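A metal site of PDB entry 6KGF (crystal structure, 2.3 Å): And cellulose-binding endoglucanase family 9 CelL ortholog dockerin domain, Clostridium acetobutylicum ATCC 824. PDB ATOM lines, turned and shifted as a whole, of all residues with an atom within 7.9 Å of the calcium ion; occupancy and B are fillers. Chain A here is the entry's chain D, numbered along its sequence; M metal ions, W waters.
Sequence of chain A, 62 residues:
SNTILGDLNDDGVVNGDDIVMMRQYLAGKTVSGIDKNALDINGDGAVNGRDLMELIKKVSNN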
ATOM      1  N   MET A  22      15.839 -17.693  15.807  1.00  0.00           N
ATOM      2  CA  MET A  22      16.570 -17.471  17.049  1.00  0.00           C
ATOM      3  C   MET A  22      15.810 -18.052  18.236  1.00  0.00           C
ATOM      4  O   MET A  22      16.382 -18.735  19.084  1.00  0.00           O
ATOM      5  CB  MET A  22      16.812 -15.975  17.252  1.00  0.00           C
ATOM      6  CG  MET A  22      17.541 -15.633  18.539  1.00  0.00           C
ATOM      7  SD  MET A  22      19.240 -16.202  18.544  1.00  0.00           S
ATOM      8  CE  MET A  22      20.025 -14.942  17.532  1.00  0.00           C
ATOM      9  N   LEU A  39      24.387 -16.499  14.488  1.00  0.00           N
ATOM     10  CA  LEU A  39      23.663 -16.468  15.757  1.00  0.00           C
ATOM     11  C   LEU A  39      24.271 -15.471  16.735  1.00  0.00           C
ATOM     12  O   LEU A  39      23.536 -14.786  17.458  1.00  0.00           O
ATOM     13  CB  LEU A  39      23.632 -17.869  16.360  1.00  0.00           C
ATOM     14  CG  LEU A  39      22.704 -18.867  15.671  1.00  0.00           C
ATOM     15  CD1 LEU A  39      23.066 -20.294  16.046  1.00  0.00           C
ATOM     16  CD2 LEU A  39      21.255 -18.579  16.025  1.00  0.00           C
ATOM     17  N   ASP A  40      25.602 -15.379  16.783  1.00  0.00           N
ATOM     18  CA  ASP A  40      26.279 -14.488  17.728  1.00  0.00           C
ATOM     19  C   ASP A  40      26.245 -13.068  17.170  1.00  0.00           C
ATOM     20  O   ASP A  40      27.160 -12.624  16.469  1.00  0.00           O
ATOM     21  CB  ASP A  40      27.709 -14.963  17.966  1.00  0.00           C
ATOM     22  CG  ASP A  40      28.379 -14.221  19.114  1.00  0.00           C
ATOM     23  OD1 ASP A  40      27.679 -13.531  19.878  1.00  0.00           O
ATOM     24  OD2 ASP A  40      29.616 -14.332  19.246  1.00  0.00           O
ATOM     25  N   ILE A  41      25.178 -12.342  17.503  1.00  0.00           N
ATOM     26  CA  ILE A  41      24.943 -11.038  16.894  1.00  0.00           C
ATOM     27  C   ILE A  41      25.796  -9.961  17.538  1.00  0.00           C
ATOM     28  O   ILE A  41      26.264  -9.032  16.858  1.00  0.00           O
ATOM     29  CB  ILE A  41      23.436 -10.700  16.975  1.00  0.00           C
ATOM     30  CG1 ILE A  41      22.659 -11.576  15.977  1.00  0.00           C
ATOM     31  CG2 ILE A  41      23.202  -9.207  16.716  1.00  0.00           C
ATOM     32  CD1 ILE A  41      21.152 -11.435  16.069  1.00  0.00           C
ATOM     33  N   ASN A  42      26.002 -10.038  18.852  1.00  0.00           N
ATOM     34  CA  ASN A  42      26.788  -9.034  19.569  1.00  0.00           C
ATOM     35  C   ASN A  42      28.252  -9.425  19.708  1.00  0.00           C
ATOM     36  O   ASN A  42      28.996  -8.729  20.414  1.00  0.00           O
ATOM     37  CB  ASN A  42      26.182  -8.775  20.951  1.00  0.00           C
ATOM     38  CG  ASN A  42      26.085 -10.033  21.794  1.00  0.00           C
ATOM     39  OD1 ASN A  42      26.753 -11.041  21.521  1.00  0.00           O
ATOM     40  ND2 ASN A  42      25.245  -9.989  22.826  1.00  0.00           N
ATOM     41  N   GLY A  43      28.690 -10.492  19.054  1.00  0.00           N
ATOM     42  CA  GLY A  43      30.091 -10.870  19.040  1.00  0.00           C
ATOM     43  C   GLY A  43      30.712 -10.944  20.415  1.00  0.00           C
ATOM     44  O   GLY A  43      31.782 -10.358  20.645  1.00  0.00           O
ATOM     45  N   ASP A  44      30.074 -11.659  21.332  1.00  0.00           N
ATOM     46  CA  ASP A  44      30.618 -11.880  22.665  1.00  0.00           C
ATOM     47  C   ASP A  44      31.008 -13.332  22.912  1.00  0.00           C
ATOM     48  O   ASP A  44      31.414 -13.674  24.028  1.00  0.00           O
ATOM     49  CB  ASP A  44      29.611 -11.421  23.734  1.00  0.00           C
ATOM     50  CG  ASP A  44      28.345 -12.269  23.754  1.00  0.00           C
ATOM     51  OD1 ASP A  44      28.227 -13.192  22.920  1.00  0.00           O
ATOM     52  OD2 ASP A  44      27.477 -12.014  24.601  1.00  0.00           O
ATOM     53  N   GLY A  45      30.913 -14.192  21.894  1.00  0.00           N
ATOM     54  CA  GLY A  45      31.364 -15.564  21.990  1.00  0.00           C
ATOM     55  C   GLY A  45      30.294 -16.573  22.361  1.00  0.00           C
ATOM     56  O   GLY A  45      30.560 -17.774  22.284  1.00  0.00           O
ATOM     57  N   ALA A  46      29.114 -16.124  22.756  1.00  0.00           N
ATOM     58  CA  ALA A  46      28.033 -17.019  23.158  1.00  0.00           C
ATOM     59  C   ALA A  46      26.767 -16.694  22.387  1.00  0.00           C
ATOM     60  O   ALA A  46      26.604 -15.597  21.848  1.00  0.00           O
ATOM     61  CB  ALA A  46      27.766 -16.934  24.664  1.00  0.00           C
ATOM     62  N   VAL A  47      25.868 -17.675  22.326  1.00  0.00           N
ATOM     63  CA  VAL A  47      24.558 -17.517  21.724  1.00  0.00           C
ATOM     64  C   VAL A  47      23.533 -17.674  22.845  1.00  0.00           C
ATOM     65  O   VAL A  47      23.335 -18.778  23.355  1.00  0.00           O
ATOM     66  CB  VAL A  47      24.300 -18.533  20.596  1.00  0.00           C
ATOM     67  CG1 VAL A  47      22.948 -18.289  19.947  1.00  0.00           C
ATOM     68  CG2 VAL A  47      25.409 -18.450  19.562  1.00  0.00           C
ATOM     69  N   ASN A  48      22.899 -16.574  23.231  1.00  0.00           N
ATOM     70  CA  ASN A  48      21.970 -16.593  24.344  1.00  0.00           C
ATOM     71  C   ASN A  48      20.905 -15.526  24.111  1.00  0.00           C
ATOM     72  O   ASN A  48      20.817 -14.923  23.029  1.00  0.00           O
ATOM     73  CB  ASN A  48      22.710 -16.396  25.677  1.00  0.00           C
ATOM     74  CG  ASN A  48      23.515 -15.111  25.705  1.00  0.00           C
ATOM     75  OD1 ASN A  48      23.219 -14.159  24.985  1.00  0.00           O
ATOM     76  ND2 ASN A  48      24.537 -15.083  26.557  1.00  0.00           N
ATOM     77  N   GLY A  49      20.085 -15.279  25.139  1.00  0.00           N
ATOM     78  CA  GLY A  49      18.964 -14.367  25.018  1.00  0.00           C
ATOM     79  C   GLY A  49      19.346 -12.940  24.641  1.00  0.00           C
ATOM     80  O   GLY A  49      18.496 -12.194  24.152  1.00  0.00           O
ATOM     81  N   ARG A  50      20.603 -12.549  24.874  1.00  0.00           N
ATOM     82  CA  ARG A  50      21.010 -11.202  24.516  1.00  0.00           C
ATOM     83  C   ARG A  50      21.230 -11.046  23.010  1.00  0.00           C
ATOM     84  O   ARG A  50      21.186  -9.922  22.502  1.00  0.00           O
ATOM     85  CB  ARG A  50      22.283 -10.815  25.265  1.00  0.00           C
ATOM     86  CG  ARG A  50      22.381  -9.326  25.531  1.00  0.00           C
ATOM     87  CD  ARG A  50      23.339  -9.023  26.673  1.00  0.00           C
ATOM     88  NE  ARG A  50      22.956  -7.781  27.350  1.00  0.00           N
ATOM     89  CZ  ARG A  50      23.598  -7.270  28.395  1.00  0.00           C
ATOM     90  NH1 ARG A  50      24.668  -7.874  28.886  1.00  0.00           N
ATOM     91  NH2 ARG A  50      23.170  -6.136  28.937  1.00  0.00           N
ATOM     92  N   ASP A  51      21.462 -12.143  22.292  1.00  0.00           N
ATOM     93  CA  ASP A  51      21.460 -12.089  20.835  1.00  0.00           C
ATOM     94  C   ASP A  51      20.047 -11.942  20.294  1.00  0.00           C
ATOM     95  O   ASP A  51      19.804 -11.215  19.334  1.00  0.00           O
ATOM     96  CB  ASP A  51      22.137 -13.334  20.267  1.00  0.00           C
ATOM     97  CG  ASP A  51      23.603 -13.423  20.631  1.00  0.00           C
ATOM     98  OD1 ASP A  51      24.377 -12.523  20.221  1.00  0.00           O
ATOM     99  OD2 ASP A  51      23.988 -14.376  21.348  1.00  0.00           O
ATOM    100  N   LEU A  52      19.081 -12.635  20.921  1.00  0.00           N
ATOM    101  CA  LEU A  52      17.677 -12.428  20.585  1.00  0.00           C
ATOM    102  C   LEU A  52      17.256 -11.000  20.884  1.00  0.00           C
ATOM    103  O   LEU A  52      16.561 -10.369  20.075  1.00  0.00           O
ATOM    104  CB  LEU A  52      16.811 -13.426  21.343  1.00  0.00           C
ATOM    105  CG  LEU A  52      15.300 -13.286  21.216  1.00  0.00           C
ATOM    106  CD1 LEU A  52      14.840 -13.441  19.773  1.00  0.00           C
ATOM    107  CD2 LEU A  52      14.599 -14.297  22.116  1.00  0.00           C
ATOM    108  N   GLU A  54      19.145  -8.338  20.888  1.00  0.00           N
ATOM    109  CA  GLU A  54      19.725  -7.484  19.862  1.00  0.00           C
ATOM    110  C   GLU A  54      18.976  -7.636  18.545  1.00  0.00           C
ATOM    111  O   GLU A  54      18.781  -6.652  17.814  1.00  0.00           O
ATOM    112  CB  GLU A  54      21.203  -7.821  19.669  1.00  0.00           C
ATOM    113  CG  GLU A  54      22.092  -7.511  20.864  1.00  0.00           C
ATOM    114  CD  GLU A  54      22.579  -6.076  20.879  1.00  0.00           C
ATOM    115  OE1 GLU A  54      21.781  -5.173  21.240  1.00  0.00           O
ATOM    116  OE2 GLU A  54      23.759  -5.850  20.539  1.00  0.00           O
HETATM  117 CA    CA M   1      26.305 -13.340  21.735  1.00  0.00          CA
HETATM  118  O   HOH W   1      25.354 -12.774  23.801  1.00  0.00           O
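The side-chain carboxylate (OD2) of Asp 40 sits at hydrogen-bond distance from the backbone NH (N) of Gly 45, 3.0 Å away.
OD1 of Asp 40 sits close to N of Gly 43.
OD1 of Asp 51 sits close to N of Ile 41, at 2.8 Å.
The backbone NH (N) of Asn 48 sits close to the side-chain carboxylate (OD2) of Asp 51 (3.1 Å).
The calcium ion is bound by OD1 of Asp 44 (2.3 Å).
The calcium ion is bound by O of Ala 46.
The calcium ion is bound by the side-chain carboxylate (OD1) of Asp 40 (2.3 Å).
Water W1 binds the calcium ion (2.3 Å).
OD1 of Asn 42 is bound to the calcium ion (2.4 Å).
The calcium ion is bound by the side-chain carboxylate (OD2) of Asp 51, at 2.6 Å.
The calcium ion is bound by OD1 of Asp 51 (2.6 Å).
The calcium ion has seven donor atoms within binding distance.
Water W1 lies within hydrogen-bond range of the side-chain amide oxygen (OD1) of Asn 48 (2.8 Å) and the side-chain amide nitrogen (ND2) of Asn 42 (3.0 Å).
Of the 16 residues printed, 5 come within 4 Å of the calcium ion.
Along chain A the residues within 4 Å of the calcium ion span positions 40 to 51.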
